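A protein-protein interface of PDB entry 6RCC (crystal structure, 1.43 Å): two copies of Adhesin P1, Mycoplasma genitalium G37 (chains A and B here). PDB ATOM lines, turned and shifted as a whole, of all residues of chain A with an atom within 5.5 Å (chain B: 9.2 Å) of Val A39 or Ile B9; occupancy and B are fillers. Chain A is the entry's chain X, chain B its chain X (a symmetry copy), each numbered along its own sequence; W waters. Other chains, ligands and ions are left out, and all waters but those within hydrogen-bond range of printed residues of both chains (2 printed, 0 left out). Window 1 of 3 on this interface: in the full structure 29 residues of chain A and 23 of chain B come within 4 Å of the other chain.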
ATOM      1  N   TYR A  34      13.883  -5.192   3.787  1.00  0.00           N
ATOM      2  CA  TYR A  34      14.116  -5.463   5.203  1.00  0.00           C
ATOM      3  C   TYR A  34      15.227  -6.445   5.480  1.00  0.00           C
ATOM      4  O   TYR A  34      15.599  -6.583   6.637  1.00  0.00           O
ATOM      5  CB  TYR A  34      12.825  -5.918   5.905  1.00  0.00           C
ATOM      6  CG  TYR A  34      11.686  -4.936   5.787  1.00  0.00           C
ATOM      7  CD1 TYR A  34      11.889  -3.568   6.012  1.00  0.00           C
ATOM      8  CD2 TYR A  34      10.406  -5.361   5.444  1.00  0.00           C
ATOM      9  CE1 TYR A  34      10.845  -2.654   5.876  1.00  0.00           C
ATOM     10  CE2 TYR A  34       9.350  -4.459   5.326  1.00  0.00           C
ATOM     11  CZ  TYR A  34       9.578  -3.104   5.546  1.00  0.00           C
ATOM     12  OH  TYR A  34       8.537  -2.216   5.403  1.00  0.00           O
ATOM     13  N   VAL A  35      15.795  -7.104   4.449  1.00  0.00           N
ATOM     14  CA  VAL A  35      16.870  -8.083   4.682  1.00  0.00           C
ATOM     15  C   VAL A  35      18.052  -7.418   5.422  1.00  0.00           C
ATOM     16  O   VAL A  35      18.475  -7.956   6.439  1.00  0.00           O
ATOM     17  CB  VAL A  35      17.279  -8.836   3.401  1.00  0.00           C
ATOM     18  CG1 VAL A  35      18.527  -9.716   3.622  1.00  0.00           C
ATOM     19  CG2 VAL A  35      16.106  -9.645   2.851  1.00  0.00           C
ATOM     20  N   PRO A  36      18.532  -6.205   5.040  1.00  0.00           N
ATOM     21  CA  PRO A  36      19.644  -5.585   5.783  1.00  0.00           C
ATOM     22  C   PRO A  36      19.301  -5.140   7.179  1.00  0.00           C
ATOM     23  O   PRO A  36      20.194  -4.895   7.990  1.00  0.00           O
ATOM     24  CB  PRO A  36      20.028  -4.363   4.936  1.00  0.00           C
ATOM     25  CG  PRO A  36      19.359  -4.532   3.664  1.00  0.00           C
ATOM     26  CD  PRO A  36      18.173  -5.389   3.861  1.00  0.00           C
ATOM     27  N   LEU A  37      18.016  -5.029   7.464  1.00  0.00           N
ATOM     28  CA  LEU A  37      17.587  -4.626   8.774  1.00  0.00           C
ATOM     29  C   LEU A  37      17.629  -5.823   9.729  1.00  0.00           C
ATOM     30  O   LEU A  37      17.965  -5.653  10.890  1.00  0.00           O
ATOM     31  CB  LEU A  37      16.164  -4.071   8.628  1.00  0.00           C
ATOM     32  CG  LEU A  37      15.514  -3.497   9.837  1.00  0.00           C
ATOM     33  CD1 LEU A  37      16.348  -2.349  10.423  1.00  0.00           C
ATOM     34  CD2 LEU A  37      14.141  -3.003   9.463  1.00  0.00           C
ATOM     35  N   LEU A  38      17.310  -7.028   9.239  1.00  0.00           N
ATOM     36  CA  LEU A  38      17.293  -8.262  10.022  1.00  0.00           C
ATOM     37  C   LEU A  38      18.628  -8.925  10.181  1.00  0.00           C
ATOM     38  O   LEU A  38      18.860  -9.632  11.173  1.00  0.00           O
ATOM     39  CB  LEU A  38      16.297  -9.269   9.418  1.00  0.00           C
ATOM     40  CG  LEU A  38      14.879  -8.720   9.229  1.00  0.00           C
ATOM     41  CD1 LEU A  38      13.955  -9.780   8.647  1.00  0.00           C
ATOM     42  CD2 LEU A  38      14.308  -8.165  10.517  1.00  0.00           C
ATOM     43  N   VAL A  39      19.480  -8.766   9.167  1.00  0.00           N
ATOM     44  CA  VAL A  39      20.792  -9.408   9.112  1.00  0.00           C
ATOM     45  C   VAL A  39      21.851  -8.332   9.040  1.00  0.00           C
ATOM     46  O   VAL A  39      21.714  -7.409   8.238  1.00  0.00           O
ATOM     47  CB  VAL A  39      20.905 -10.354   7.898  1.00  0.00           C
ATOM     48  CG1 VAL A  39      22.252 -11.083   7.902  1.00  0.00           C
ATOM     49  CG2 VAL A  39      19.768 -11.372   7.905  1.00  0.00           C
ATOM     50  N   ASN A  40      22.902  -8.457   9.870  1.00  0.00           N
ATOM     51  CA  ASN A  40      24.016  -7.536   9.853  1.00  0.00           C
ATOM     52  C   ASN A  40      24.938  -7.969   8.710  1.00  0.00           C
ATOM     53  O   ASN A  40      25.692  -8.949   8.827  1.00  0.00           O
ATOM     54  CB  ASN A  40      24.755  -7.611  11.166  1.00  0.00           C
ATOM     55  CG  ASN A  40      25.854  -6.597  11.284  1.00  0.00           C
ATOM     56  OD1 ASN A  40      25.861  -5.555  10.603  1.00  0.00           O
ATOM     57  ND2 ASN A  40      26.810  -6.894  12.151  1.00  0.00           N
ATOM     58  N   LEU A  41      24.790  -7.289   7.589  1.00  0.00           N
ATOM     59  CA  LEU A  41      25.544  -7.601   6.389  1.00  0.00           C
ATOM     60  C   LEU A  41      26.902  -6.974   6.377  1.00  0.00           C
ATOM     61  O   LEU A  41      27.068  -5.818   6.776  1.00  0.00           O
ATOM     62  CB  LEU A  41      24.779  -7.144   5.140  1.00  0.00           C
ATOM     63  CG  LEU A  41      23.384  -7.736   4.940  1.00  0.00           C
ATOM     64  CD1 LEU A  41      22.651  -7.041   3.813  1.00  0.00           C
ATOM     65  CD2 LEU A  41      23.430  -9.258   4.722  1.00  0.00           C
ATOM     66  N   LEU A  52      15.739 -14.423   2.470  1.00  0.00           N
ATOM     67  CA  LEU A  52      15.412 -15.015   3.773  1.00  0.00           C
ATOM     68  C   LEU A  52      14.048 -15.610   3.732  1.00  0.00           C
ATOM     69  O   LEU A  52      13.079 -14.895   3.512  1.00  0.00           O
ATOM     70  CB  LEU A  52      15.438 -13.970   4.904  1.00  0.00           C
ATOM     71  CG  LEU A  52      16.746 -13.358   5.252  1.00  0.00           C
ATOM     72  CD1 LEU A  52      16.531 -12.260   6.321  1.00  0.00           C
ATOM     73  CD2 LEU A  52      17.695 -14.426   5.832  1.00  0.00           C
ATOM     74  N   THR A  91      17.431 -19.707  12.531  1.00  0.00           N
ATOM     75  CA  THR A  91      17.405 -18.823  13.684  1.00  0.00           C
ATOM     76  C   THR A  91      15.999 -18.381  13.992  1.00  0.00           C
ATOM     77  O   THR A  91      15.214 -18.171  13.055  1.00  0.00           O
ATOM     78  CB  THR A  91      18.355 -17.617  13.491  1.00  0.00           C
ATOM     79  OG1 THR A  91      18.363 -16.838  14.693  1.00  0.00           O
ATOM     80  CG2 THR A  91      18.003 -16.770  12.289  1.00  0.00           C
ATOM     81  N   PHE A  93      14.327 -15.279  16.222  1.00  0.00           N
ATOM     82  CA  PHE A  93      14.727 -14.057  16.895  1.00  0.00           C
ATOM     83  C   PHE A  93      13.613 -13.032  16.910  1.00  0.00           C
ATOM     84  O   PHE A  93      12.655 -13.115  16.113  1.00  0.00           O
ATOM     85  CB  PHE A  93      16.018 -13.498  16.237  1.00  0.00           C
ATOM     86  CG  PHE A  93      15.838 -12.943  14.855  1.00  0.00           C
ATOM     87  CD1 PHE A  93      15.579 -13.782  13.777  1.00  0.00           C
ATOM     88  CD2 PHE A  93      15.946 -11.579  14.621  1.00  0.00           C
ATOM     89  CE1 PHE A  93      15.384 -13.257  12.489  1.00  0.00           C
ATOM     90  CE2 PHE A  93      15.811 -11.069  13.325  1.00  0.00           C
ATOM     91  CZ  PHE A  93      15.502 -11.907  12.273  1.00  0.00           C
ATOM     92  N   GLY B   6      15.503  -6.399  21.008  1.00  0.00           N
ATOM     93  CA  GLY B   6      15.503  -7.216  19.820  1.00  0.00           C
ATOM     94  C   GLY B   6      16.916  -7.577  19.400  1.00  0.00           C
ATOM     95  O   GLY B   6      17.888  -7.331  20.114  1.00  0.00           O
ATOM     96  N   ASN B   7      17.036  -8.168  18.215  1.00  0.00           N
ATOM     97  CA  ASN B   7      18.341  -8.540  17.686  1.00  0.00           C
ATOM     98  C   ASN B   7      18.354  -8.488  16.177  1.00  0.00           C
ATOM     99  O   ASN B   7      17.355  -8.785  15.511  1.00  0.00           O
ATOM    100  CB  ASN B   7      18.767  -9.938  18.129  1.00  0.00           C
ATOM    101  CG  ASN B   7      19.709  -9.927  19.309  1.00  0.00           C
ATOM    102  OD1 ASN B   7      20.613  -9.106  19.418  1.00  0.00           O
ATOM    103  ND2 ASN B   7      19.539 -10.846  20.205  1.00  0.00           N
ATOM    104  N   GLN B   8      19.538  -8.222  15.647  1.00  0.00           N
ATOM    105  CA  GLN B   8      19.850  -8.232  14.233  1.00  0.00           C
ATOM    106  C   GLN B   8      20.853  -9.421  14.184  1.00  0.00           C
ATOM    107  O   GLN B   8      21.774  -9.476  15.012  1.00  0.00           O
ATOM    108  CB  GLN B   8      20.549  -6.931  13.843  1.00  0.00           C
ATOM    109  CG  GLN B   8      20.854  -6.843  12.357  1.00  0.00           C
ATOM    110  CD  GLN B   8      21.697  -5.624  12.017  1.00  0.00           C
ATOM    111  OE1 GLN B   8      22.689  -5.312  12.713  1.00  0.00           O
ATOM    112  NE2 GLN B   8      21.369  -4.952  10.895  1.00  0.00           N
ATOM    113  N   ILE B   9      20.669 -10.373  13.271  1.00  0.00           N
ATOM    114  CA  ILE B   9      21.489 -11.570  13.236  1.00  0.00           C
ATOM    115  C   ILE B   9      22.788 -11.333  12.498  1.00  0.00           C
ATOM    116  O   ILE B   9      22.760 -10.813  11.387  1.00  0.00           O
ATOM    117  CB  ILE B   9      20.712 -12.744  12.554  1.00  0.00           C
ATOM    118  CG1 ILE B   9      19.340 -12.986  13.202  1.00  0.00           C
ATOM    119  CG2 ILE B   9      21.547 -14.052  12.472  1.00  0.00           C
ATOM    120  CD1 ILE B   9      19.443 -13.376  14.754  1.00  0.00           C
ATOM    121  N   ASP B  10      23.889 -11.786  13.053  1.00  0.00           N
ATOM    122  CA  ASP B  10      25.142 -11.691  12.338  1.00  0.00           C
ATOM    123  C   ASP B  10      25.135 -12.616  11.145  1.00  0.00           C
ATOM    124  O   ASP B  10      24.714 -13.784  11.233  1.00  0.00           O
ATOM    125  CB  ASP B  10      26.324 -11.997  13.255  1.00  0.00           C
ATOM    126  CG  ASP B  10      26.634 -10.865  14.220  1.00  0.00           C
ATOM    127  OD1 ASP B  10      26.363  -9.687  13.868  1.00  0.00           O
ATOM    128  OD2 ASP B  10      27.167 -11.151  15.316  1.00  0.00           O
ATOM    129  N   PHE B  11      25.602 -12.103  10.009  1.00  0.00           N
ATOM    130  CA  PHE B  11      25.625 -12.903   8.796  1.00  0.00           C
ATOM    131  C   PHE B  11      26.327 -14.271   8.970  1.00  0.00           C
ATOM    132  O   PHE B  11      25.844 -15.240   8.398  1.00  0.00           O
ATOM    133  CB  PHE B  11      26.285 -12.098   7.655  1.00  0.00           C
ATOM    134  CG  PHE B  11      26.109 -12.678   6.280  1.00  0.00           C
ATOM    135  CD1 PHE B  11      24.867 -12.687   5.665  1.00  0.00           C
ATOM    136  CD2 PHE B  11      27.187 -13.212   5.600  1.00  0.00           C
ATOM    137  CE1 PHE B  11      24.704 -13.233   4.384  1.00  0.00           C
ATOM    138  CE2 PHE B  11      27.028 -13.729   4.311  1.00  0.00           C
ATOM    139  CZ  PHE B  11      25.795 -13.732   3.710  1.00  0.00           C
ATOM    140  N   ASN B  12      27.400 -14.345   9.772  1.00  0.00           N
ATOM    141  CA  ASN B  12      28.172 -15.580   9.972  1.00  0.00           C
ATOM    142  C   ASN B  12      27.428 -16.665  10.771  1.00  0.00           C
ATOM    143  O   ASN B  12      27.879 -17.812  10.832  1.00  0.00           O
ATOM    144  CB  ASN B  12      29.548 -15.285  10.573  1.00  0.00           C
ATOM    145  CG  ASN B  12      29.570 -14.707  11.970  1.00  0.00           C
ATOM    146  OD1 ASN B  12      28.550 -14.583  12.660  1.00  0.00           O
ATOM    147  ND2 ASN B  12      30.758 -14.346  12.423  1.00  0.00           N
ATOM    148  N   ARG B  13      26.274 -16.322  11.358  1.00  0.00           N
ATOM    149  CA  ARG B  13      25.433 -17.309  12.016  1.00  0.00           C
ATOM    150  C   ARG B  13      24.561 -18.031  11.005  1.00  0.00           C
ATOM    151  O   ARG B  13      24.005 -19.081  11.323  1.00  0.00           O
ATOM    152  CB  ARG B  13      24.521 -16.655  13.076  1.00  0.00           C
ATOM    153  CG  ARG B  13      25.277 -16.071  14.257  1.00  0.00           C
ATOM    154  CD  ARG B  13      25.762 -17.165  15.186  1.00  0.00           C
ATOM    155  NE  ARG B  13      26.506 -16.610  16.319  1.00  0.00           N
ATOM    156  CZ  ARG B  13      27.006 -17.354  17.302  1.00  0.00           C
ATOM    157  NH1 ARG B  13      26.848 -18.671  17.291  1.00  0.00           N
ATOM    158  NH2 ARG B  13      27.662 -16.787  18.300  1.00  0.00           N
ATOM    159  N   LEU B  14      24.389 -17.442   9.788  1.00  0.00           N
ATOM    160  CA  LEU B  14      23.500 -17.988   8.769  1.00  0.00           C
ATOM    161  C   LEU B  14      24.222 -18.533   7.567  1.00  0.00           C
ATOM    162  O   LEU B  14      23.652 -19.356   6.839  1.00  0.00           O
ATOM    163  CB  LEU B  14      22.570 -16.869   8.295  1.00  0.00           C
ATOM    164  CG  LEU B  14      21.617 -16.309   9.362  1.00  0.00           C
ATOM    165  CD1 LEU B  14      20.916 -15.119   8.847  1.00  0.00           C
ATOM    166  CD2 LEU B  14      20.597 -17.346   9.783  1.00  0.00           C
ATOM    167  N   PHE B  15      25.421 -18.016   7.295  1.00  0.00           N
ATOM    168  CA  PHE B  15      26.092 -18.367   6.066  1.00  0.00           C
ATOM    169  C   PHE B  15      27.466 -18.934   6.291  1.00  0.00           C
ATOM    170  O   PHE B  15      28.255 -18.368   7.038  1.00  0.00           O
ATOM    171  CB  PHE B  15      26.200 -17.100   5.179  1.00  0.00           C
ATOM    172  CG  PHE B  15      26.762 -17.374   3.802  1.00  0.00           C
ATOM    173  CD1 PHE B  15      25.952 -17.887   2.791  1.00  0.00           C
ATOM    174  CD2 PHE B  15      28.115 -17.198   3.541  1.00  0.00           C
ATOM    175  CE1 PHE B  15      26.492 -18.196   1.527  1.00  0.00           C
ATOM    176  CE2 PHE B  15      28.643 -17.487   2.276  1.00  0.00           C
ATOM    177  CZ  PHE B  15      27.835 -17.996   1.290  1.00  0.00           C
HETATM  178  O   HOH W   1      24.045  -3.617   9.670  1.00  0.00           O
HETATM  179  O   HOH W   2      16.403  -6.951  13.538  1.00  0.00           O
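The backbone carbonyl oxygen (O) of Pro A36 is in hydrogen-bond range of the side-chain amide nitrogen (NE2) of Gln B8, at 3.1 Å.
O of Leu A37 sits close to NE2 of Gln B8 (3.5 Å).
The backbone carbonyl oxygen (O) of Ile B9 sits at hydrogen-bond distance from the backbone NH (N) of Asn A40 (2.8 Å).
The backbone NH (N) of Ile B9 lies within hydrogen-bond range of the backbone carbonyl oxygen (O) of Leu A38 (2.9 Å).
The side-chain amide nitrogen of Asn A40 sits at hydrogen-bond distance from the side-chain carboxylate of Asp B10 (3.3 Å).
The backbone carbonyl oxygen (O) of Asn A40 is in hydrogen-bond range of the backbone NH (N) of Phe B11, at 3.4 Å.
Among the printed residues, merely in contact across the chains: Phe A93 with Asn B7 (3.3 Å), Val A39 with Ile B9 (3.3 Å), Asn A40 with Gln B8 (3.5 Å), Leu A38 with Gln B8 (3.5 Å), Thr A91 with Ile B9 (3.6 Å), Phe A93 with Ile B9 (3.6 Å), Val A39 with Gln B8 (3.6 Å), Thr A91 with Leu B14 (3.7 Å), Val A39 with Phe B11 (3.8 Å) and Leu A41 with Phe B11 (3.8 Å).
Of the printed residues of chain B, Pro A36 touches Gln B8.
Of the printed residues of chain B, Leu A38 touches Gln B8 and Ile B9.
Of the printed residues of chain B, Asn A40 touches Gln B8 (3.5 Å), Ile B9 (2.8 Å), Asp B10 (3.3 Å) and Phe B11 (3.4 Å).
Of the printed residues of chain A, Phe B11 touches Val A39 (3.8 Å), Asn A40 (3.4 Å) and Leu A41 (3.8 Å).
Phe B15 touches none of the printed residues of chain A.
The nearest printed residue of chain B that does not touch Val A39 is Leu B14 (4.03 Å).
Among the printed residues, 16 pairs touch across the chains.
Among the printed residues, no Asp or Glu carboxylate lies within 4 Å of a Lys or Arg side-chain nitrogen of the other chain.
No position is printed for both chains.
Of the 16 pairs that touch across the chains among the printed residues, none has its exchanged pair printed and touching as well.
Water W1 lies within hydrogen-bond range of OD1 of Asn A40 and NE2 of Gln B8.
Water W2 bridges the backbone carbonyl oxygen (O) of Asn B7 (2.9 Å) and the backbone carbonyl oxygen (O) of Leu A37 (3.3 Å).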
